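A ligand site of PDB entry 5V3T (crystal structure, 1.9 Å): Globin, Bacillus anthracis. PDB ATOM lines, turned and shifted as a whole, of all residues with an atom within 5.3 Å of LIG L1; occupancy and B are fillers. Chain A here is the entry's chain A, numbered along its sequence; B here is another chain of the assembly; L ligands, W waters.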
ATOM      1  N   LEU A  35     -26.885 -17.616 -10.016  1.00  0.00           N
ATOM      2  CA  LEU A  35     -27.349 -16.776  -8.911  1.00  0.00           C
ATOM      3  C   LEU A  35     -28.830 -16.397  -9.005  1.00  0.00           C
ATOM      4  O   LEU A  35     -29.552 -16.493  -8.014  1.00  0.00           O
ATOM      5  CB  LEU A  35     -26.513 -15.512  -8.836  1.00  0.00           C
ATOM      6  CG  LEU A  35     -25.017 -15.701  -8.561  1.00  0.00           C
ATOM      7  CD1 LEU A  35     -24.365 -14.329  -8.494  1.00  0.00           C
ATOM      8  CD2 LEU A  35     -24.805 -16.472  -7.259  1.00  0.00           C
ATOM      9  N   ILE A  38     -31.989 -18.203  -7.207  1.00  0.00           N
ATOM     10  CA  ILE A  38     -32.218 -18.293  -5.771  1.00  0.00           C
ATOM     11  C   ILE A  38     -32.574 -16.936  -5.184  1.00  0.00           C
ATOM     12  O   ILE A  38     -32.980 -16.845  -4.024  1.00  0.00           O
ATOM     13  CB  ILE A  38     -31.008 -18.880  -5.016  1.00  0.00           C
ATOM     14  CG1 ILE A  38     -29.757 -18.046  -5.228  1.00  0.00           C
ATOM     15  CG2 ILE A  38     -30.750 -20.283  -5.482  1.00  0.00           C
ATOM     16  CD1 ILE A  38     -28.514 -18.686  -4.626  1.00  0.00           C
ATOM     17  N   PHE A  39     -32.469 -15.896  -5.999  1.00  0.00           N
ATOM     18  CA  PHE A  39     -32.899 -14.570  -5.591  1.00  0.00           C
ATOM     19  C   PHE A  39     -34.371 -14.314  -5.861  1.00  0.00           C
ATOM     20  O   PHE A  39     -34.963 -14.941  -6.739  1.00  0.00           O
ATOM     21  CB  PHE A  39     -32.052 -13.525  -6.316  1.00  0.00           C
ATOM     22  CG  PHE A  39     -30.690 -13.391  -5.745  1.00  0.00           C
ATOM     23  CD1 PHE A  39     -30.477 -12.586  -4.656  1.00  0.00           C
ATOM     24  CD2 PHE A  39     -29.632 -14.112  -6.271  1.00  0.00           C
ATOM     25  CE1 PHE A  39     -29.237 -12.478  -4.126  1.00  0.00           C
ATOM     26  CE2 PHE A  39     -28.386 -14.013  -5.733  1.00  0.00           C
ATOM     27  CZ  PHE A  39     -28.177 -13.193  -4.660  1.00  0.00           C
ATOM     28  N   PRO A  40     -34.976 -13.369  -5.111  1.00  0.00           N
ATOM     29  CA  PRO A  40     -36.341 -12.963  -5.437  1.00  0.00           C
ATOM     30  C   PRO A  40     -36.386 -12.423  -6.865  1.00  0.00           C
ATOM     31  O   PRO A  40     -35.383 -11.913  -7.342  1.00  0.00           O
ATOM     32  CB  PRO A  40     -36.654 -11.884  -4.398  1.00  0.00           C
ATOM     33  CG  PRO A  40     -35.714 -12.171  -3.261  1.00  0.00           C
ATOM     34  CD  PRO A  40     -34.462 -12.698  -3.908  1.00  0.00           C
ATOM     35  N   GLU A  45     -35.905  -4.701  -3.326  1.00  0.00           N
ATOM     36  CA  GLU A  45     -35.777  -4.690  -1.870  1.00  0.00           C
ATOM     37  C   GLU A  45     -34.416  -5.242  -1.431  1.00  0.00           C
ATOM     38  O   GLU A  45     -33.794  -4.720  -0.499  1.00  0.00           O
ATOM     39  CB  GLU A  45     -36.928  -5.483  -1.227  1.00  0.00           C
ATOM     40  CG  GLU A  45     -36.809  -5.622   0.285  1.00  0.00           C
ATOM     41  CD  GLU A  45     -36.867  -4.301   1.043  1.00  0.00           C
ATOM     42  OE1 GLU A  45     -37.153  -3.231   0.431  1.00  0.00           O
ATOM     43  OE2 GLU A  45     -36.609  -4.314   2.261  1.00  0.00           O
ATOM     44  N   THR A  46     -33.940  -6.262  -2.144  1.00  0.00           N
ATOM     45  CA  THR A  46     -32.596  -6.806  -1.885  1.00  0.00           C
ATOM     46  C   THR A  46     -31.516  -5.750  -2.135  1.00  0.00           C
ATOM     47  O   THR A  46     -30.583  -5.591  -1.328  1.00  0.00           O
ATOM     48  CB  THR A  46     -32.332  -8.046  -2.762  1.00  0.00           C
ATOM     49  OG1 THR A  46     -33.342  -9.029  -2.510  1.00  0.00           O
ATOM     50  CG2 THR A  46     -30.959  -8.640  -2.451  1.00  0.00           C
ATOM     51  N   LYS A  49     -31.565  -3.104   0.626  1.00  0.00           N
ATOM     52  CA  LYS A  49     -30.983  -3.631   1.848  1.00  0.00           C
ATOM     53  C   LYS A  49     -29.473  -3.738   1.748  1.00  0.00           C
ATOM     54  O   LYS A  49     -28.763  -3.461   2.707  1.00  0.00           O
ATOM     55  CB  LYS A  49     -31.612  -4.993   2.212  1.00  0.00           C
ATOM     56  CG  LYS A  49     -33.024  -4.861   2.796  1.00  0.00           C
ATOM     57  CD  LYS A  49     -33.615  -6.202   3.266  1.00  0.00           C
ATOM     58  CE  LYS A  49     -33.970  -7.099   2.094  1.00  0.00           C
ATOM     59  NZ  LYS A  49     -34.797  -8.288   2.503  1.00  0.00           N
ATOM     60  N   GLN A  50     -28.989  -4.144   0.575  1.00  0.00           N
ATOM     61  CA  GLN A  50     -27.547  -4.299   0.362  1.00  0.00           C
ATOM     62  C   GLN A  50     -26.838  -2.940   0.442  1.00  0.00           C
ATOM     63  O   GLN A  50     -25.708  -2.856   0.924  1.00  0.00           O
ATOM     64  CB  GLN A  50     -27.267  -4.966  -0.989  1.00  0.00           C
ATOM     65  CG  GLN A  50     -25.786  -5.232  -1.241  1.00  0.00           C
ATOM     66  CD  GLN A  50     -25.237  -6.342  -0.359  1.00  0.00           C
ATOM     67  OE1 GLN A  50     -24.772  -6.119   0.761  1.00  0.00           O
ATOM     68  NE2 GLN A  50     -25.312  -7.552  -0.857  1.00  0.00           N
ATOM     69  N   PHE A  53     -26.539  -2.267   3.993  1.00  0.00           N
ATOM     70  CA  PHE A  53     -25.511  -3.106   4.599  1.00  0.00           C
ATOM     71  C   PHE A  53     -24.088  -2.666   4.249  1.00  0.00           C
ATOM     72  O   PHE A  53     -23.256  -2.459   5.141  1.00  0.00           O
ATOM     73  CB  PHE A  53     -25.673  -4.595   4.228  1.00  0.00           C
ATOM     74  CG  PHE A  53     -24.621  -5.448   4.860  1.00  0.00           C
ATOM     75  CD1 PHE A  53     -24.721  -5.805   6.193  1.00  0.00           C
ATOM     76  CD2 PHE A  53     -23.511  -5.827   4.160  1.00  0.00           C
ATOM     77  CE1 PHE A  53     -23.724  -6.556   6.798  1.00  0.00           C
ATOM     78  CE2 PHE A  53     -22.509  -6.597   4.754  1.00  0.00           C
ATOM     79  CZ  PHE A  53     -22.620  -6.958   6.080  1.00  0.00           C
ATOM     80  N   LEU A  54     -23.815  -2.492   2.969  1.00  0.00           N
ATOM     81  CA  LEU A  54     -22.471  -2.115   2.544  1.00  0.00           C
ATOM     82  C   LEU A  54     -22.040  -0.761   3.105  1.00  0.00           C
ATOM     83  O   LEU A  54     -20.858  -0.554   3.372  1.00  0.00           O
ATOM     84  CB  LEU A  54     -22.361  -2.089   1.015  1.00  0.00           C
ATOM     85  CG  LEU A  54     -22.467  -3.483   0.398  1.00  0.00           C
ATOM     86  CD1 LEU A  54     -22.354  -3.420  -1.128  1.00  0.00           C
ATOM     87  CD2 LEU A  54     -21.399  -4.403   0.962  1.00  0.00           C
ATOM     88  N   TYR A  64     -28.168  -0.381   8.234  1.00  0.00           N
ATOM     89  CA  TYR A  64     -28.743  -1.720   8.247  1.00  0.00           C
ATOM     90  C   TYR A  64     -29.250  -2.050   9.646  1.00  0.00           C
ATOM     91  O   TYR A  64     -30.420  -2.394   9.815  1.00  0.00           O
ATOM     92  CB  TYR A  64     -27.722  -2.767   7.808  1.00  0.00           C
ATOM     93  CG  TYR A  64     -28.326  -4.170   7.699  1.00  0.00           C
ATOM     94  CD1 TYR A  64     -28.470  -4.977   8.822  1.00  0.00           C
ATOM     95  CD2 TYR A  64     -28.762  -4.669   6.470  1.00  0.00           C
ATOM     96  CE1 TYR A  64     -29.025  -6.245   8.726  1.00  0.00           C
ATOM     97  CE2 TYR A  64     -29.324  -5.957   6.370  1.00  0.00           C
ATOM     98  CZ  TYR A  64     -29.457  -6.728   7.509  1.00  0.00           C
ATOM     99  OH  TYR A  64     -30.004  -7.997   7.428  1.00  0.00           O
ATOM    100  N   HIS A  68     -32.935  -3.152  10.551  1.00  0.00           N
ATOM    101  CA  HIS A  68     -33.136  -4.596  10.443  1.00  0.00           C
ATOM    102  C   HIS A  68     -32.564  -5.401  11.605  1.00  0.00           C
ATOM    103  O   HIS A  68     -32.747  -6.618  11.680  1.00  0.00           O
ATOM    104  CB  HIS A  68     -32.481  -5.105   9.147  1.00  0.00           C
ATOM    105  CG  HIS A  68     -32.891  -4.347   7.925  1.00  0.00           C
ATOM    106  ND1 HIS A  68     -34.121  -4.513   7.319  1.00  0.00           N
ATOM    107  CD2 HIS A  68     -32.237  -3.418   7.196  1.00  0.00           C
ATOM    108  CE1 HIS A  68     -34.198  -3.727   6.262  1.00  0.00           C
ATOM    109  NE2 HIS A  68     -33.072  -3.045   6.163  1.00  0.00           N
ATOM    110  N   LEU A  73     -24.961 -12.365   9.145  1.00  0.00           N
ATOM    111  CA  LEU A  73     -25.206 -12.727   7.753  1.00  0.00           C
ATOM    112  C   LEU A  73     -25.215 -14.213   7.537  1.00  0.00           C
ATOM    113  O   LEU A  73     -26.041 -14.706   6.765  1.00  0.00           O
ATOM    114  CB  LEU A  73     -24.190 -12.073   6.840  1.00  0.00           C
ATOM    115  CG  LEU A  73     -24.484 -10.612   6.494  1.00  0.00           C
ATOM    116  CD1 LEU A  73     -23.698 -10.227   5.258  1.00  0.00           C
ATOM    117  CD2 LEU A  73     -25.995 -10.388   6.276  1.00  0.00           C
ATOM    118  N   ARG A  76     -28.485 -15.499   8.435  1.00  0.00           N
ATOM    119  CA  ARG A  76     -29.520 -15.084   7.495  1.00  0.00           C
ATOM    120  C   ARG A  76     -29.466 -15.810   6.142  1.00  0.00           C
ATOM    121  O   ARG A  76     -30.470 -15.869   5.430  1.00  0.00           O
ATOM    122  CB  ARG A  76     -29.445 -13.579   7.249  1.00  0.00           C
ATOM    123  CG  ARG A  76     -29.759 -12.730   8.471  1.00  0.00           C
ATOM    124  CD  ARG A  76     -29.861 -11.267   8.060  1.00  0.00           C
ATOM    125  NE  ARG A  76     -30.003 -10.357   9.200  1.00  0.00           N
ATOM    126  CZ  ARG A  76     -31.171  -9.858   9.614  1.00  0.00           C
ATOM    127  NH1 ARG A  76     -31.220  -9.027  10.644  1.00  0.00           N
ATOM    128  NH2 ARG A  76     -32.288 -10.172   8.959  1.00  0.00           N
ATOM    129  N   HIS A  77     -28.313 -16.377   5.816  1.00  0.00           N
ATOM    130  CA  HIS A  77     -28.138 -17.122   4.561  1.00  0.00           C
ATOM    131  C   HIS A  77     -28.305 -18.629   4.680  1.00  0.00           C
ATOM    132  O   HIS A  77     -28.198 -19.349   3.688  1.00  0.00           O
ATOM    133  CB  HIS A  77     -26.759 -16.822   3.977  1.00  0.00           C
ATOM    134  CG  HIS A  77     -26.660 -15.477   3.340  1.00  0.00           C
ATOM    135  ND1 HIS A  77     -26.456 -14.330   4.064  1.00  0.00           N
ATOM    136  CD2 HIS A  77     -26.721 -15.107   2.043  1.00  0.00           C
ATOM    137  CE1 HIS A  77     -26.395 -13.296   3.240  1.00  0.00           C
ATOM    138  NE2 HIS A  77     -26.550 -13.736   2.009  1.00  0.00           N
ATOM    139  N   PHE A  80     -30.522 -20.750   2.253  1.00  0.00           N
ATOM    140  CA  PHE A  80     -30.234 -20.675   0.817  1.00  0.00           C
ATOM    141  C   PHE A  80     -29.068 -21.575   0.425  1.00  0.00           C
ATOM    142  O   PHE A  80     -28.144 -21.796   1.214  1.00  0.00           O
ATOM    143  CB  PHE A  80     -29.955 -19.230   0.401  1.00  0.00           C
ATOM    144  CG  PHE A  80     -30.989 -18.254   0.899  1.00  0.00           C
ATOM    145  CD1 PHE A  80     -32.313 -18.366   0.514  1.00  0.00           C
ATOM    146  CD2 PHE A  80     -30.617 -17.198   1.728  1.00  0.00           C
ATOM    147  CE1 PHE A  80     -33.262 -17.467   0.966  1.00  0.00           C
ATOM    148  CE2 PHE A  80     -31.561 -16.286   2.178  1.00  0.00           C
ATOM    149  CZ  PHE A  80     -32.883 -16.421   1.789  1.00  0.00           C
ATOM    150  N   GLU A  81     -29.127 -22.125  -0.783  1.00  0.00           N
ATOM    151  CA  GLU A  81     -28.095 -23.055  -1.223  1.00  0.00           C
ATOM    152  C   GLU A  81     -26.854 -22.306  -1.681  1.00  0.00           C
ATOM    153  O   GLU A  81     -26.708 -22.033  -2.863  1.00  0.00           O
ATOM    154  CB  GLU A  81     -28.625 -23.947  -2.345  1.00  0.00           C
ATOM    155  CG  GLU A  81     -27.637 -25.017  -2.762  1.00  0.00           C
ATOM    156  CD  GLU A  81     -28.232 -26.025  -3.722  1.00  0.00           C
ATOM    157  OE1 GLU A  81     -28.807 -25.585  -4.745  1.00  0.00           O
ATOM    158  OE2 GLU A  81     -28.149 -27.238  -3.448  1.00  0.00           O
ATOM    159  N   ILE A  82     -25.967 -21.993  -0.743  1.00  0.00           N
ATOM    160  CA  ILE A  82     -24.754 -21.250  -1.088  1.00  0.00           C
ATOM    161  C   ILE A  82     -23.575 -22.211  -1.169  1.00  0.00           C
ATOM    162  O   ILE A  82     -22.954 -22.597  -0.178  1.00  0.00           O
ATOM    163  CB  ILE A  82     -24.490 -20.131  -0.075  1.00  0.00           C
ATOM    164  CG1 ILE A  82     -25.728 -19.259   0.036  1.00  0.00           C
ATOM    165  CG2 ILE A  82     -23.262 -19.291  -0.512  1.00  0.00           C
ATOM    166  CD1 ILE A  82     -25.551 -18.095   0.942  1.00  0.00           C
ATOM    167  N   ARG A  86     -21.317 -20.808  -6.057  1.00  0.00           N
ATOM    168  CA  ARG A  86     -22.122 -19.610  -6.032  1.00  0.00           C
ATOM    169  C   ARG A  86     -21.411 -18.461  -5.313  1.00  0.00           C
ATOM    170  O   ARG A  86     -21.565 -17.301  -5.692  1.00  0.00           O
ATOM    171  CB  ARG A  86     -23.484 -19.903  -5.398  1.00  0.00           C
ATOM    172  CG  ARG A  86     -24.338 -20.752  -6.307  1.00  0.00           C
ATOM    173  CD  ARG A  86     -25.725 -20.969  -5.757  1.00  0.00           C
ATOM    174  NE  ARG A  86     -26.612 -21.462  -6.799  1.00  0.00           N
ATOM    175  CZ  ARG A  86     -27.548 -22.383  -6.615  1.00  0.00           C
ATOM    176  NH1 ARG A  86     -27.703 -22.933  -5.416  1.00  0.00           N
ATOM    177  NH2 ARG A  86     -28.313 -22.766  -7.621  1.00  0.00           N
ATOM    178  N   ALA A  87     -20.628 -18.775  -4.285  1.00  0.00           N
ATOM    179  CA  ALA A  87     -19.789 -17.748  -3.667  1.00  0.00           C
ATOM    180  C   ALA A  87     -18.848 -17.172  -4.718  1.00  0.00           C
ATOM    181  O   ALA A  87     -18.618 -15.963  -4.767  1.00  0.00           O
ATOM    182  CB  ALA A  87     -19.016 -18.322  -2.481  1.00  0.00           C
ATOM    183  N   TRP A  90     -20.858 -14.887  -7.053  1.00  0.00           N
ATOM    184  CA  TRP A  90     -21.173 -13.649  -6.367  1.00  0.00           C
ATOM    185  C   TRP A  90     -20.012 -12.667  -6.456  1.00  0.00           C
ATOM    186  O   TRP A  90     -20.189 -11.504  -6.816  1.00  0.00           O
ATOM    187  CB  TRP A  90     -21.473 -13.943  -4.886  1.00  0.00           C
ATOM    188  CG  TRP A  90     -22.136 -12.851  -4.183  1.00  0.00           C
ATOM    189  CD1 TRP A  90     -23.462 -12.734  -3.977  1.00  0.00           C
ATOM    190  CD2 TRP A  90     -21.525 -11.691  -3.573  1.00  0.00           C
ATOM    191  NE1 TRP A  90     -23.720 -11.593  -3.272  1.00  0.00           N
ATOM    192  CE2 TRP A  90     -22.564 -10.934  -3.001  1.00  0.00           C
ATOM    193  CE3 TRP A  90     -20.210 -11.231  -3.447  1.00  0.00           C
ATOM    194  CZ2 TRP A  90     -22.341  -9.721  -2.313  1.00  0.00           C
ATOM    195  CZ3 TRP A  90     -19.980 -10.030  -2.764  1.00  0.00           C
ATOM    196  CH2 TRP A  90     -21.045  -9.287  -2.199  1.00  0.00           C
ATOM    197  N   LEU A 115     -15.084  -8.582   1.365  1.00  0.00           N
ATOM    198  CA  LEU A 115     -16.227  -9.260   0.774  1.00  0.00           C
ATOM    199  C   LEU A 115     -15.944 -10.737   0.485  1.00  0.00           C
ATOM    200  O   LEU A 115     -16.820 -11.592   0.650  1.00  0.00           O
ATOM    201  CB  LEU A 115     -16.640  -8.531  -0.508  1.00  0.00           C
ATOM    202  CG  LEU A 115     -17.266  -7.148  -0.331  1.00  0.00           C
ATOM    203  CD1 LEU A 115     -17.637  -6.556  -1.669  1.00  0.00           C
ATOM    204  CD2 LEU A 115     -18.492  -7.284   0.535  1.00  0.00           C
ATOM    205  N   THR A 118     -16.190 -12.588   3.727  1.00  0.00           N
ATOM    206  CA  THR A 118     -17.603 -12.709   4.090  1.00  0.00           C
ATOM    207  C   THR A 118     -18.332 -13.753   3.232  1.00  0.00           C
ATOM    208  O   THR A 118     -19.109 -14.569   3.735  1.00  0.00           O
ATOM    209  CB  THR A 118     -18.333 -11.368   3.949  1.00  0.00           C
ATOM    210  OG1 THR A 118     -17.754 -10.420   4.859  1.00  0.00           O
ATOM    211  CG2 THR A 118     -19.808 -11.523   4.276  1.00  0.00           C
ATOM    212  N   ALA A 119     -18.104 -13.710   1.918  1.00  0.00           N
ATOM    213  CA  ALA A 119     -18.747 -14.656   1.010  1.00  0.00           C
ATOM    214  C   ALA A 119     -18.368 -16.100   1.325  1.00  0.00           C
ATOM    215  O   ALA A 119     -19.207 -17.010   1.206  1.00  0.00           O
ATOM    216  CB  ALA A 119     -18.393 -14.317  -0.431  1.00  0.00           C
ATOM    217  N   MET A 122     -20.431 -17.360   4.194  1.00  0.00           N
ATOM    218  CA  MET A 122     -21.812 -17.646   3.831  1.00  0.00           C
ATOM    219  C   MET A 122     -22.012 -19.084   3.313  1.00  0.00           C
ATOM    220  O   MET A 122     -23.093 -19.634   3.447  1.00  0.00           O
ATOM    221  CB  MET A 122     -22.317 -16.648   2.782  1.00  0.00           C
ATOM    222  CG  MET A 122     -22.227 -15.175   3.165  1.00  0.00           C
ATOM    223  SD  MET A 122     -23.145 -14.838   4.673  1.00  0.00           S
ATOM    224  CE  MET A 122     -21.789 -14.768   5.868  1.00  0.00           C
ATOM    225  N   ARG B 114     -39.671 -14.707   4.628  1.00  0.00           N
ATOM    226  CA  ARG B 114     -38.433 -15.466   4.508  1.00  0.00           C
ATOM    227  C   ARG B 114     -38.695 -16.966   4.374  1.00  0.00           C
ATOM    228  O   ARG B 114     -38.026 -17.635   3.590  1.00  0.00           O
ATOM    229  CB  ARG B 114     -37.546 -15.175   5.715  1.00  0.00           C
ATOM    230  CG  ARG B 114     -37.034 -13.755   5.592  1.00  0.00           C
ATOM    231  CD  ARG B 114     -36.266 -13.297   6.795  1.00  0.00           C
ATOM    232  NE  ARG B 114     -35.621 -12.009   6.501  1.00  0.00           N
ATOM    233  CZ  ARG B 114     -36.275 -10.878   6.253  1.00  0.00           C
ATOM    234  NH1 ARG B 114     -37.604 -10.836   6.261  1.00  0.00           N
ATOM    235  NH2 ARG B 114     -35.595  -9.765   6.015  1.00  0.00           N
ATOM    236  N   LEU B 117     -40.057 -17.682   0.786  1.00  0.00           N
ATOM    237  CA  LEU B 117     -38.953 -17.731  -0.170  1.00  0.00           C
ATOM    238  C   LEU B 117     -38.195 -19.050  -0.016  1.00  0.00           C
ATOM    239  O   LEU B 117     -37.855 -19.691  -1.002  1.00  0.00           O
ATOM    240  CB  LEU B 117     -37.993 -16.553   0.034  1.00  0.00           C
ATOM    241  CG  LEU B 117     -36.752 -16.503  -0.861  1.00  0.00           C
ATOM    242  CD1 LEU B 117     -37.144 -16.422  -2.342  1.00  0.00           C
ATOM    243  CD2 LEU B 117     -35.855 -15.342  -0.474  1.00  0.00           C
ATOM    244  N   HIS B 121     -37.614 -22.349  -2.621  1.00  0.00           N
ATOM    245  CA  HIS B 121     -36.304 -22.921  -2.928  1.00  0.00           C
ATOM    246  C   HIS B 121     -36.258 -24.433  -2.728  1.00  0.00           C
ATOM    247  O   HIS B 121     -35.493 -25.117  -3.382  1.00  0.00           O
ATOM    248  CB  HIS B 121     -35.200 -22.259  -2.080  1.00  0.00           C
ATOM    249  CG  HIS B 121     -34.871 -20.857  -2.508  1.00  0.00           C
ATOM    250  ND1 HIS B 121     -35.632 -20.157  -3.418  1.00  0.00           N
ATOM    251  CD2 HIS B 121     -33.848 -20.039  -2.161  1.00  0.00           C
ATOM    252  CE1 HIS B 121     -35.098 -18.960  -3.614  1.00  0.00           C
ATOM    253  NE2 HIS B 121     -34.010 -18.867  -2.858  1.00  0.00           N
HETATM  254  C1  LIG L   1     -29.793 -11.797   1.407  1.00  0.00           C
HETATM  255  C2  LIG L   1     -27.696 -15.057  -1.670  1.00  0.00           C
HETATM  256  C3  LIG L   1     -23.321 -13.556  -0.102  1.00  0.00           C
HETATM  257  C4  LIG L   1     -25.307  -9.740   2.216  1.00  0.00           C
HETATM  258  C5  LIG L   1     -29.585 -12.788   0.441  1.00  0.00           C
HETATM  259  C6  LIG L   1     -30.640 -13.519  -0.243  1.00  0.00           C
HETATM  260  C7  LIG L   1     -30.076 -14.405  -1.083  1.00  0.00           C
HETATM  261  C8  LIG L   1     -28.629 -14.288  -0.969  1.00  0.00           C
HETATM  262  C9  LIG L   1     -30.815 -15.385  -2.015  1.00  0.00           C
HETATM  263  C10 LIG L   1     -32.156 -13.284  -0.054  1.00  0.00           C
HETATM  264  C11 LIG L   1     -32.505 -11.869  -0.520  1.00  0.00           C
HETATM  265  C12 LIG L   1     -33.626 -11.302   0.310  1.00  0.00           C
HETATM  266  O1  LIG L   1     -34.302 -12.097   1.011  1.00  0.00           O
HETATM  267  O2  LIG L   1     -33.839 -10.065   0.273  1.00  0.00           O
HETATM  268  C13 LIG L   1     -26.327 -14.956  -1.495  1.00  0.00           C
HETATM  269  C14 LIG L   1     -25.301 -15.768  -2.125  1.00  0.00           C
HETATM  270  C15 LIG L   1     -24.112 -15.360  -1.671  1.00  0.00           C
HETATM  271  C16 LIG L   1     -24.317 -14.259  -0.742  1.00  0.00           C
HETATM  272  C17 LIG L   1     -25.551 -16.929  -3.123  1.00  0.00           C
HETATM  273  C18 LIG L   1     -22.738 -15.937  -2.072  1.00  0.00           C
HETATM  274  C19 LIG L   1     -21.735 -16.024  -1.182  1.00  0.00           C
HETATM  275  C20 LIG L   1     -23.474 -12.356   0.545  1.00  0.00           C
HETATM  276  C21 LIG L   1     -22.408 -11.427   0.871  1.00  0.00           C
HETATM  277  C22 LIG L   1     -22.958 -10.380   1.496  1.00  0.00           C
HETATM  278  C23 LIG L   1     -24.388 -10.599   1.613  1.00  0.00           C
HETATM  279  C24 LIG L   1     -20.902 -11.587   0.564  1.00  0.00           C
HETATM  280  C25 LIG L   1     -22.147  -9.169   2.028  1.00  0.00           C
HETATM  281  C26 LIG L   1     -22.686  -7.977   1.895  1.00  0.00           C
HETATM  282  C27 LIG L   1     -26.694  -9.953   2.199  1.00  0.00           C
HETATM  283  C28 LIG L   1     -27.651  -9.069   2.831  1.00  0.00           C
HETATM  284  C29 LIG L   1     -29.024  -9.692   2.602  1.00  0.00           C
HETATM  285  C30 LIG L   1     -28.796 -10.905   1.834  1.00  0.00           C
HETATM  286  C31 LIG L   1     -27.335  -7.754   3.590  1.00  0.00           C
HETATM  287  C32 LIG L   1     -30.375  -9.116   3.077  1.00  0.00           C
HETATM  288  C33 LIG L   1     -30.846  -9.941   4.263  1.00  0.00           C
HETATM  289  C34 LIG L   1     -32.020  -9.279   4.947  1.00  0.00           C
HETATM  290  O3  LIG L   1     -33.152  -9.766   4.731  1.00  0.00           O
HETATM  291  O4  LIG L   1     -31.823  -8.286   5.700  1.00  0.00           O
HETATM  292  N1  LIG L   1     -28.369 -13.288  -0.019  1.00  0.00           N
HETATM  293  N2  LIG L   1     -25.674 -14.039  -0.668  1.00  0.00           N
HETATM  294  N3  LIG L   1     -24.677 -11.824   0.994  1.00  0.00           N
HETATM  295  N4  LIG L   1     -27.409 -11.030   1.634  1.00  0.00           N
HETATM  296 FE1  LIG L   1     -26.533 -12.437   0.362  1.00  0.00          FE
HETATM  297  C1  LG2 L   2     -26.637 -11.202  -1.184  1.00  0.00           C
HETATM  298  N1  LG2 L   2     -26.690 -10.584  -2.158  1.00  0.00           N
HETATM  299  O   HOH W   1     -33.066 -12.515   3.721  1.00  0.00           O
HETATM  300  O   HOH W   2     -33.628  -8.035   7.584  1.00  0.00           O
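N1 of LG2 L2 sits at hydrogen-bond distance from NE1 of Trp 90 (3.3 Å). The guanidinium group (NH2) of Arg 76 lies within salt-bridge range of an oxygen (O4) of LIG L1 (3.8 Å). The side-chain amino group (NZ) of Lys 49 is in salt-bridge range of an oxygen (O2) of LIG L1, at 3.0 Å. A ring nitrogen (NE2) of His 77 is bound to an iron atom (FE1) of LIG L1. OH of Tyr 64 is in hydrogen-bond range of O4 of LIG L1 (2.5 Å). An oxygen (O2) of LIG L1 sits at hydrogen-bond distance from the side-chain hydroxyl (OG1) of Thr 46 (3.0 Å). O3 of LIG L1 is in salt-bridge range of NH2 of Arg 114 of chain B (2.8 Å).
The backbone carbonyl oxygen of Ile 38 lies within hydrogen-bond range of a ring nitrogen (NE2) of His 121 of chain B. ND1 of His 77 lies within hydrogen-bond range of SD of Met 122, at 3.4 Å. A ring nitrogen (ND1) of His 77 lies within hydrogen-bond range of the backbone carbonyl oxygen of Leu 73 (2.8 Å). O of His 68 is in hydrogen-bond range of NH1 of Arg 76, at 3.0 Å. ND1 of His 121 of chain B sits at hydrogen-bond distance from O of Leu 117 of chain B, at 3.3 Å. NE of Arg 76 is in hydrogen-bond range of OH of Tyr 64.
Ile 38 touches LIG L1 (O to C9, 3.3 Å). CZ of Phe 39 touches C2 of LIG L1 (3.6 Å). Pro 40 touches LIG L1. Gln 50 touches LIG L1. Phe 53 touches LIG L1 (CE2 to C26, 3.2 Å). Leu 54 touches LIG L1 (CD2 to C26, 3.9 Å). CD1 of Leu 73 touches C4 of LIG L1, at 3.5 Å. Phe 80 touches LIG L1. CG2 of Ile 82 touches C19 of LIG L1, 3.7 Å away. CA of Ala 87 touches C19 of LIG L1, 3.6 Å away. Trp 90 touches LIG L1. Thr 118 touches LIG L1. Ala 119 touches LIG L1 (O to C19, 3.6 Å). CG of Met 122 touches C3 of LIG L1 (3.8 Å). Leu 117 of chain B touches LIG L1. Hydrophobic or aromatic side chains that line LIG L1: Ile 38, Phe 39, Pro 40, Phe 53, Leu 54, Tyr 64, Leu 73, His 77, Phe 80, Ile 82, Ala 87, Trp 90, Ala 119, Met 122 and Leu 117 of chain B.
Water W2 lies within hydrogen-bond range of O4 of LIG L1 (2.6 Å), NH2 of Arg 76 (2.9 Å) and NH2 of Arg 114 of chain B (3.1 Å).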
